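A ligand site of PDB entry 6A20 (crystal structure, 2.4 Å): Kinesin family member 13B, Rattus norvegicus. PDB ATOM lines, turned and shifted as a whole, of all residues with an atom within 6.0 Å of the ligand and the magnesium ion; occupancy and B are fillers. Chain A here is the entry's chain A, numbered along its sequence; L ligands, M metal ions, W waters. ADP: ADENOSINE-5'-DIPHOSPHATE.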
ATOM      1  N   ARG A  11     -30.693 -10.595 -14.485  1.00  0.00           N
ATOM      2  CA  ARG A  11     -29.873 -10.532 -13.289  1.00  0.00           C
ATOM      3  C   ARG A  11     -29.254  -9.143 -13.119  1.00  0.00           C
ATOM      4  O   ARG A  11     -28.494  -8.679 -13.966  1.00  0.00           O
ATOM      5  CB  ARG A  11     -28.772 -11.594 -13.320  1.00  0.00           C
ATOM      6  CG  ARG A  11     -28.101 -11.811 -11.968  1.00  0.00           C
ATOM      7  CD  ARG A  11     -27.058 -12.910 -12.026  1.00  0.00           C
ATOM      8  NE  ARG A  11     -26.632 -13.303 -10.686  1.00  0.00           N
ATOM      9  CZ  ARG A  11     -25.591 -14.098 -10.436  1.00  0.00           C
ATOM     10  NH1 ARG A  11     -25.295 -14.406  -9.180  1.00  0.00           N
ATOM     11  NH2 ARG A  11     -24.860 -14.576 -11.426  1.00  0.00           N
ATOM     12  N   VAL A  12     -29.599  -8.489 -12.018  1.00  0.00           N
ATOM     13  CA  VAL A  12     -29.063  -7.178 -11.695  1.00  0.00           C
ATOM     14  C   VAL A  12     -27.943  -7.299 -10.685  1.00  0.00           C
ATOM     15  O   VAL A  12     -28.170  -7.666  -9.538  1.00  0.00           O
ATOM     16  CB  VAL A  12     -30.155  -6.236 -11.134  1.00  0.00           C
ATOM     17  CG1 VAL A  12     -29.613  -4.815 -11.020  1.00  0.00           C
ATOM     18  CG2 VAL A  12     -31.390  -6.276 -12.011  1.00  0.00           C
ATOM     19  N   ARG A  13     -26.718  -6.993 -11.109  1.00  0.00           N
ATOM     20  CA  ARG A  13     -25.580  -7.040 -10.193  1.00  0.00           C
ATOM     21  C   ARG A  13     -25.670  -5.885  -9.197  1.00  0.00           C
ATOM     22  O   ARG A  13     -26.187  -4.813  -9.537  1.00  0.00           O
ATOM     23  CB  ARG A  13     -24.259  -6.996 -10.965  1.00  0.00           C
ATOM     24  CG  ARG A  13     -23.947  -5.666 -11.635  1.00  0.00           C
ATOM     25  CD  ARG A  13     -22.455  -5.516 -11.886  1.00  0.00           C
ATOM     26  NE  ARG A  13     -22.129  -4.254 -12.550  1.00  0.00           N
ATOM     27  CZ  ARG A  13     -22.008  -3.095 -11.917  1.00  0.00           C
ATOM     28  NH1 ARG A  13     -22.184  -3.025 -10.605  1.00  0.00           N
ATOM     29  NH2 ARG A  13     -21.708  -1.998 -12.602  1.00  0.00           N
ATOM     30  N   PRO A  14     -25.184  -6.099  -7.977  1.00  0.00           N
ATOM     31  CA  PRO A  14     -25.238  -5.058  -6.946  1.00  0.00           C
ATOM     32  C   PRO A  14     -24.313  -3.888  -7.253  1.00  0.00           C
ATOM     33  O   PRO A  14     -23.375  -4.033  -8.024  1.00  0.00           O
ATOM     34  CB  PRO A  14     -24.786  -5.790  -5.683  1.00  0.00           C
ATOM     35  CG  PRO A  14     -23.939  -6.911  -6.173  1.00  0.00           C
ATOM     36  CD  PRO A  14     -24.575  -7.342  -7.467  1.00  0.00           C
ATOM     37  N   SER A  64     -29.291  -8.549  -5.716  1.00  0.00           N
ATOM     38  CA  SER A  64     -28.535  -8.692  -4.479  1.00  0.00           C
ATOM     39  C   SER A  64     -28.485  -7.365  -3.721  1.00  0.00           C
ATOM     40  O   SER A  64     -28.391  -6.307  -4.334  1.00  0.00           O
ATOM     41  CB  SER A  64     -27.120  -9.192  -4.763  1.00  0.00           C
ATOM     42  OG  SER A  64     -27.146 -10.500  -5.319  1.00  0.00           O
ATOM     43  N   ASP A  66     -26.126  -6.439  -1.524  1.00  0.00           N
ATOM     44  CA  ASP A  66     -24.754  -5.937  -1.435  1.00  0.00           C
ATOM     45  C   ASP A  66     -23.754  -6.896  -2.087  1.00  0.00           C
ATOM     46  O   ASP A  66     -24.137  -7.867  -2.736  1.00  0.00           O
ATOM     47  CB  ASP A  66     -24.376  -5.693   0.023  1.00  0.00           C
ATOM     48  CG  ASP A  66     -24.652  -6.888   0.927  1.00  0.00           C
ATOM     49  OD1 ASP A  66     -25.164  -6.671   2.046  1.00  0.00           O
ATOM     50  OD2 ASP A  66     -24.363  -8.033   0.521  1.00  0.00           O
ATOM     51  N   GLU A  67     -22.471  -6.611  -1.900  1.00  0.00           N
ATOM     52  CA  GLU A  67     -21.407  -7.421  -2.480  1.00  0.00           C
ATOM     53  C   GLU A  67     -20.735  -8.335  -1.454  1.00  0.00           C
ATOM     54  O   GLU A  67     -19.651  -8.852  -1.692  1.00  0.00           O
ATOM     55  CB  GLU A  67     -20.347  -6.528  -3.129  1.00  0.00           C
ATOM     56  CG  GLU A  67     -20.690  -6.070  -4.534  1.00  0.00           C
ATOM     57  CD  GLU A  67     -19.545  -5.322  -5.192  1.00  0.00           C
ATOM     58  OE1 GLU A  67     -19.266  -5.578  -6.383  1.00  0.00           O
ATOM     59  OE2 GLU A  67     -18.918  -4.462  -4.514  1.00  0.00           O
ATOM     60  N   LYS A  72     -23.407 -13.069  -2.332  1.00  0.00           N
ATOM     61  CA  LYS A  72     -22.874 -13.593  -3.580  1.00  0.00           C
ATOM     62  C   LYS A  72     -23.088 -15.108  -3.669  1.00  0.00           C
ATOM     63  O   LYS A  72     -23.514 -15.627  -4.699  1.00  0.00           O
ATOM     64  CB  LYS A  72     -21.394 -13.253  -3.728  1.00  0.00           C
ATOM     65  CG  LYS A  72     -21.119 -11.748  -3.726  1.00  0.00           C
ATOM     66  CD  LYS A  72     -19.639 -11.435  -3.837  1.00  0.00           C
ATOM     67  CE  LYS A  72     -19.134 -11.610  -5.258  1.00  0.00           C
ATOM     68  NZ  LYS A  72     -17.737 -11.129  -5.407  1.00  0.00           N
ATOM     69  N   GLN A  76     -25.398 -16.910  -6.525  1.00  0.00           N
ATOM     70  CA  GLN A  76     -25.029 -17.998  -7.420  1.00  0.00           C
ATOM     71  C   GLN A  76     -25.911 -19.221  -7.179  1.00  0.00           C
ATOM     72  O   GLN A  76     -26.383 -19.866  -8.139  1.00  0.00           O
ATOM     73  CB  GLN A  76     -23.554 -18.371  -7.229  1.00  0.00           C
ATOM     74  CG  GLN A  76     -22.569 -17.250  -7.544  1.00  0.00           C
ATOM     75  CD  GLN A  76     -22.491 -16.907  -9.020  1.00  0.00           C
ATOM     76  OE1 GLN A  76     -23.470 -16.460  -9.624  1.00  0.00           O
ATOM     77  NE2 GLN A  76     -21.333 -17.142  -9.616  1.00  0.00           N
ATOM     78  N   GLY A 103     -25.696  -9.070 -22.303  1.00  0.00           N
ATOM     79  CA  GLY A 103     -25.584  -7.833 -21.564  1.00  0.00           C
ATOM     80  C   GLY A 103     -24.269  -7.119 -21.822  1.00  0.00           C
ATOM     81  O   GLY A 103     -23.356  -7.677 -22.431  1.00  0.00           O
ATOM     82  N   GLN A 104     -24.177  -5.875 -21.346  1.00  0.00           N
ATOM     83  CA  GLN A 104     -22.979  -5.072 -21.560  1.00  0.00           C
ATOM     84  C   GLN A 104     -21.812  -5.561 -20.722  1.00  0.00           C
ATOM     85  O   GLN A 104     -21.990  -6.315 -19.760  1.00  0.00           O
ATOM     86  CB  GLN A 104     -23.270  -3.600 -21.227  1.00  0.00           C
ATOM     87  CG  GLN A 104     -23.565  -3.363 -19.763  1.00  0.00           C
ATOM     88  CD  GLN A 104     -23.640  -1.884 -19.425  1.00  0.00           C
ATOM     89  OE1 GLN A 104     -24.426  -1.476 -18.570  1.00  0.00           O
ATOM     90  NE2 GLN A 104     -22.829  -1.077 -20.090  1.00  0.00           N
ATOM     91  N   THR A 105     -20.602  -5.146 -21.093  1.00  0.00           N
ATOM     92  CA  THR A 105     -19.398  -5.523 -20.378  1.00  0.00           C
ATOM     93  C   THR A 105     -19.431  -5.017 -18.937  1.00  0.00           C
ATOM     94  O   THR A 105     -19.639  -3.830 -18.687  1.00  0.00           O
ATOM     95  CB  THR A 105     -18.132  -4.990 -21.079  1.00  0.00           C
ATOM     96  OG1 THR A 105     -18.042  -5.552 -22.386  1.00  0.00           O
ATOM     97  CG2 THR A 105     -16.883  -5.346 -20.285  1.00  0.00           C
ATOM     98  N   GLY A 106     -19.224  -5.932 -17.994  1.00  0.00           N
ATOM     99  CA  GLY A 106     -19.220  -5.573 -16.582  1.00  0.00           C
ATOM    100  C   GLY A 106     -20.560  -5.773 -15.902  1.00  0.00           C
ATOM    101  O   GLY A 106     -20.710  -5.455 -14.718  1.00  0.00           O
ATOM    102  N   SER A 107     -21.539  -6.283 -16.646  1.00  0.00           N
ATOM    103  CA  SER A 107     -22.872  -6.503 -16.093  1.00  0.00           C
ATOM    104  C   SER A 107     -22.943  -7.804 -15.298  1.00  0.00           C
ATOM    105  O   SER A 107     -23.690  -7.894 -14.315  1.00  0.00           O
ATOM    106  CB  SER A 107     -23.925  -6.500 -17.199  1.00  0.00           C
ATOM    107  OG  SER A 107     -23.610  -7.433 -18.212  1.00  0.00           O
ATOM    108  N   GLY A 108     -22.187  -8.806 -15.721  1.00  0.00           N
ATOM    109  CA  GLY A 108     -22.107 -10.050 -14.984  1.00  0.00           C
ATOM    110  C   GLY A 108     -22.326 -11.317 -15.798  1.00  0.00           C
ATOM    111  O   GLY A 108     -22.791 -12.319 -15.256  1.00  0.00           O
ATOM    112  N   LYS A 109     -22.004 -11.276 -17.084  1.00  0.00           N
ATOM    113  CA  LYS A 109     -22.171 -12.434 -17.957  1.00  0.00           C
ATOM    114  C   LYS A 109     -21.246 -13.588 -17.536  1.00  0.00           C
ATOM    115  O   LYS A 109     -21.718 -14.696 -17.251  1.00  0.00           O
ATOM    116  CB  LYS A 109     -21.889 -12.065 -19.417  1.00  0.00           C
ATOM    117  CG  LYS A 109     -22.887 -11.088 -20.012  1.00  0.00           C
ATOM    118  CD  LYS A 109     -22.589 -10.827 -21.480  1.00  0.00           C
ATOM    119  CE  LYS A 109     -21.241 -10.143 -21.669  1.00  0.00           C
ATOM    120  NZ  LYS A 109     -21.183  -8.822 -20.986  1.00  0.00           N
ATOM    121  N   SER A 110     -19.950 -13.309 -17.492  1.00  0.00           N
ATOM    122  CA  SER A 110     -18.970 -14.324 -17.135  1.00  0.00           C
ATOM    123  C   SER A 110     -19.109 -14.761 -15.690  1.00  0.00           C
ATOM    124  O   SER A 110     -18.926 -15.936 -15.362  1.00  0.00           O
ATOM    125  CB  SER A 110     -17.553 -13.802 -17.396  1.00  0.00           C
ATOM    126  OG  SER A 110     -17.380 -13.451 -18.752  1.00  0.00           O
ATOM    127  N   TYR A 111     -19.441 -13.815 -14.814  1.00  0.00           N
ATOM    128  CA  TYR A 111     -19.655 -14.109 -13.404  1.00  0.00           C
ATOM    129  C   TYR A 111     -20.845 -15.051 -13.216  1.00  0.00           C
ATOM    130  O   TYR A 111     -20.890 -15.832 -12.259  1.00  0.00           O
ATOM    131  CB  TYR A 111     -19.882 -12.816 -12.614  1.00  0.00           C
ATOM    132  CG  TYR A 111     -20.195 -13.031 -11.152  1.00  0.00           C
ATOM    133  CD1 TYR A 111     -19.175 -13.217 -10.219  1.00  0.00           C
ATOM    134  CD2 TYR A 111     -21.513 -13.052 -10.693  1.00  0.00           C
ATOM    135  CE1 TYR A 111     -19.469 -13.416  -8.876  1.00  0.00           C
ATOM    136  CE2 TYR A 111     -21.804 -13.247  -9.363  1.00  0.00           C
ATOM    137  CZ  TYR A 111     -20.774 -13.430  -8.465  1.00  0.00           C
ATOM    138  OH  TYR A 111     -21.068 -13.629  -7.122  1.00  0.00           O
ATOM    139  N   THR A 112     -21.804 -14.985 -14.141  1.00  0.00           N
ATOM    140  CA  THR A 112     -22.978 -15.849 -14.085  1.00  0.00           C
ATOM    141  C   THR A 112     -22.669 -17.217 -14.678  1.00  0.00           C
ATOM    142  O   THR A 112     -22.975 -18.252 -14.075  1.00  0.00           O
ATOM    143  CB  THR A 112     -24.170 -15.228 -14.827  1.00  0.00           C
ATOM    144  OG1 THR A 112     -24.583 -14.035 -14.148  1.00  0.00           O
ATOM    145  CG2 THR A 112     -25.334 -16.197 -14.885  1.00  0.00           C
ATOM    146  N   THR A 116     -16.343 -17.158 -10.359  1.00  0.00           N
ATOM    147  CA  THR A 116     -14.963 -17.074  -9.904  1.00  0.00           C
ATOM    148  C   THR A 116     -14.584 -18.293  -9.073  1.00  0.00           C
ATOM    149  O   THR A 116     -15.379 -19.223  -8.938  1.00  0.00           O
ATOM    150  CB  THR A 116     -14.718 -15.800  -9.065  1.00  0.00           C
ATOM    151  OG1 THR A 116     -15.526 -15.831  -7.896  1.00  0.00           O
ATOM    152  CG2 THR A 116     -15.047 -14.562  -9.885  1.00  0.00           C
ATOM    153  N   ASP A 253     -21.440 -17.618 -23.260  1.00  0.00           N
ATOM    154  CA  ASP A 253     -21.070 -16.316 -22.724  1.00  0.00           C
ATOM    155  C   ASP A 253     -20.783 -15.357 -23.867  1.00  0.00           C
ATOM    156  O   ASP A 253     -19.713 -15.396 -24.471  1.00  0.00           O
ATOM    157  CB  ASP A 253     -19.846 -16.445 -21.803  1.00  0.00           C
ATOM    158  CG  ASP A 253     -19.432 -15.122 -21.188  1.00  0.00           C
ATOM    159  OD1 ASP A 253     -20.225 -14.162 -21.223  1.00  0.00           O
ATOM    160  OD2 ASP A 253     -18.294 -15.039 -20.666  1.00  0.00           O
ATOM    161  N   LEU A 254     -21.757 -14.508 -24.168  1.00  0.00           N
ATOM    162  CA  LEU A 254     -21.687 -13.632 -25.333  1.00  0.00           C
ATOM    163  C   LEU A 254     -20.738 -12.450 -25.134  1.00  0.00           C
ATOM    164  O   LEU A 254     -20.257 -12.207 -24.024  1.00  0.00           O
ATOM    165  CB  LEU A 254     -23.081 -13.109 -25.693  1.00  0.00           C
ATOM    166  CG  LEU A 254     -24.104 -14.168 -26.102  1.00  0.00           C
ATOM    167  CD1 LEU A 254     -25.490 -13.570 -26.130  1.00  0.00           C
ATOM    168  CD2 LEU A 254     -23.737 -14.758 -27.452  1.00  0.00           C
ATOM    169  N   THR A 329     -27.978  -9.891 -18.046  1.00  0.00           N
ATOM    170  CA  THR A 329     -27.301  -9.236 -16.946  1.00  0.00           C
ATOM    171  C   THR A 329     -27.270  -7.721 -17.172  1.00  0.00           C
ATOM    172  O   THR A 329     -26.964  -7.269 -18.280  1.00  0.00           O
ATOM    173  CB  THR A 329     -25.876  -9.763 -16.763  1.00  0.00           C
ATOM    174  OG1 THR A 329     -25.120  -9.532 -17.959  1.00  0.00           O
ATOM    175  CG2 THR A 329     -25.900 -11.260 -16.476  1.00  0.00           C
HETATM  176  PB  ADP L   1     -19.099  -9.266 -17.940  1.00  0.00           P
HETATM  177  O1B ADP L   1     -18.640 -10.664 -18.221  1.00  0.00           O
HETATM  178  O2B ADP L   1     -18.172  -8.319 -18.531  1.00  0.00           O
HETATM  179  O3B ADP L   1     -20.470  -9.065 -18.525  1.00  0.00           O
HETATM  180  PA  ADP L   1     -18.266  -9.827 -15.340  1.00  0.00           P
HETATM  181  O1A ADP L   1     -18.753 -11.271 -15.256  1.00  0.00           O
HETATM  182  O2A ADP L   1     -16.788  -9.803 -15.779  1.00  0.00           O
HETATM  183  O3A ADP L   1     -19.165  -9.044 -16.398  1.00  0.00           O
HETATM  184  O5' ADP L   1     -18.420  -9.142 -13.905  1.00  0.00           O
HETATM  185  C5' ADP L   1     -17.474  -8.145 -13.490  1.00  0.00           C
HETATM  186  C4' ADP L   1     -17.312  -8.208 -11.909  1.00  0.00           C
HETATM  187  O4' ADP L   1     -18.486  -7.452 -11.229  1.00  0.00           O
HETATM  188  C3' ADP L   1     -17.397  -9.417 -11.502  1.00  0.00           C
HETATM  189  O3' ADP L   1     -16.046  -9.989 -11.321  1.00  0.00           O
HETATM  190  C2' ADP L   1     -18.180  -9.366 -10.071  1.00  0.00           C
HETATM  191  O2' ADP L   1     -17.233  -9.058  -8.993  1.00  0.00           O
HETATM  192  C1' ADP L   1     -19.060  -8.428 -10.181  1.00  0.00           C
HETATM  193  N9  ADP L   1     -20.315  -8.942 -10.632  1.00  0.00           N
HETATM  194  C8  ADP L   1     -20.901  -9.142 -11.810  1.00  0.00           C
HETATM  195  N7  ADP L   1     -22.117  -9.669 -11.529  1.00  0.00           N
HETATM  196  C5  ADP L   1     -22.251  -9.772 -10.183  1.00  0.00           C
HETATM  197  C6  ADP L   1     -23.301 -10.247  -9.377  1.00  0.00           C
HETATM  198  N6  ADP L   1     -24.573 -10.768  -9.758  1.00  0.00           N
HETATM  199  N1  ADP L   1     -23.167 -10.247  -8.043  1.00  0.00           N
HETATM  200  C2  ADP L   1     -22.017  -9.787  -7.469  1.00  0.00           C
HETATM  201  N3  ADP L   1     -20.997  -9.323  -8.241  1.00  0.00           N
HETATM  202  C4  ADP L   1     -21.132  -9.319  -9.611  1.00  0.00           C
HETATM  203 MG    MG M   1     -17.106 -11.485 -19.347  1.00  0.00          MG
HETATM  204  O   HOH W   1     -15.649 -10.989  -7.843  1.00  0.00           O
HETATM  205  O   HOH W   2     -16.436  -9.582 -20.277  1.00  0.00           O
HETATM  206  O   HOH W   3     -18.586  -8.458  -6.797  1.00  0.00           O
HETATM  207  O   HOH W   4     -15.416 -12.062 -20.493  1.00  0.00           O
HETATM  208  O   HOH W   5     -18.188 -11.997 -21.035  1.00  0.00           O
HETATM  209  O   HOH W   6     -19.075  -4.493 -10.400  1.00  0.00           O
HETATM  210  O   HOH W   7     -15.606 -10.928 -17.841  1.00  0.00           O
HETATM  211  O   HOH W   8     -16.000  -7.084 -17.232  1.00  0.00           O
HETATM  212  O   HOH W   9     -24.629 -11.838  -6.045  1.00  0.00           O
HETATM  213  O   HOH W  10     -16.088 -12.446 -13.464  1.00  0.00           O
HETATM  214  O   HOH W  11     -27.457 -10.266  -8.168  1.00  0.00           O
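N6 of the ligand lies close to NE of Arg 11 (3.4 Å).
The backbone carbonyl oxygen (O) of Gln 104 lies close to an oxygen (O3B) of the ligand (3.4 Å).
Arg 13 touches the ligand.
CD of Pro 14 touches N1 of the ligand, at 3.3 Å.
Thr 105 touches the ligand (C to O2B, 3.6 Å).
Ser 107 touches the ligand (N to O3B, 3.5 Å).
Hydrophobic or aromatic side chains within 4 Å of the ligand: Pro 14 and Tyr 111.
Of the 23 residues printed, 11 come within 4 Å of the ligand.
Along chain A the residues within 4 Å of the ligand span positions 11 to 111.
Asp 253 touches the magnesium ion.
Within 4 Å of the magnesium ion: Ser 110 and Asp 253.
OE1 of Gln 76 lies within hydrogen-bond range of NH1 of Arg 11, 2.8 Å away.
O of Gln 104 is in hydrogen-bond range of OG of Ser 107 (2.5 Å).
O of Gly 106 sits at hydrogen-bond distance from NE of Arg 13.
OG of Ser 107 sits at hydrogen-bond distance from OG1 of Thr 329 (2.6 Å).
The side-chain hydroxyl of Thr 112 sits at hydrogen-bond distance from the guanidinium group of Arg 11 (2.8 Å).
The side-chain hydroxyl of Ser 110 lies close to the side-chain carboxylate of Asp 253 (2.6 Å).
NZ of Lys 109 lies within hydrogen-bond range of O of Gln 104 (2.9 Å).
The side-chain hydroxyl of Thr 112 is in hydrogen-bond range of the backbone carbonyl oxygen of Gly 108 (2.7 Å).
Water W3 lies within hydrogen-bond range of O2' of the ligand (2.6 Å), OE1 of Glu 67 (3.0 Å) and NZ of Lys 72 (3.1 Å).
Water W1 bridges O2' of the ligand (2.7 Å) and NZ of Lys 72 (3.2 Å).
Water W9 lies within hydrogen-bond range of OG of Ser 64 and N1 of the ligand.
Water W6 lies within hydrogen-bond range of an oxygen (O4') of the ligand (3.1 Å) and the guanidinium group (NH1) of Arg 13 (3.4 Å).
Water W11 lies within hydrogen-bond range of the side-chain hydroxyl (OG) of Ser 64 (2.9 Å), the backbone carbonyl oxygen (O) of Val 12 (3.0 Å) and a nitrogen (N6) of the ligand (3.3 Å).
The backbone NH (N) of Gly 108 sits at hydrogen-bond distance from an oxygen (O3A) of the ligand (3.1 Å).
An oxygen (O1A) of the ligand sits at hydrogen-bond distance from the backbone NH of Ser 110, at 3.3 Å.
N of Lys 109 lies within hydrogen-bond range of O3B of the ligand (3.1 Å).
N of Tyr 111 is in hydrogen-bond range of O1A of the ligand, 2.7 Å away.
The side-chain amino group (NZ) of Lys 109 is in salt-bridge range of an oxygen (O3B) of the ligand.
The backbone NH (N) of Gly 106 is in hydrogen-bond range of an oxygen (O2B) of the ligand (2.7 Å).
The magnesium ion is bound by water W5 (2.1 Å), the side-chain hydroxyl (OG) of Ser 110 (2.1 Å), an oxygen (O1B) of the ligand (2.1 Å), water W4 (2.1 Å), water W7 (2.2 Å) and water W2 (2.2 Å).
The magnesium ion has six donor atoms within binding distance.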
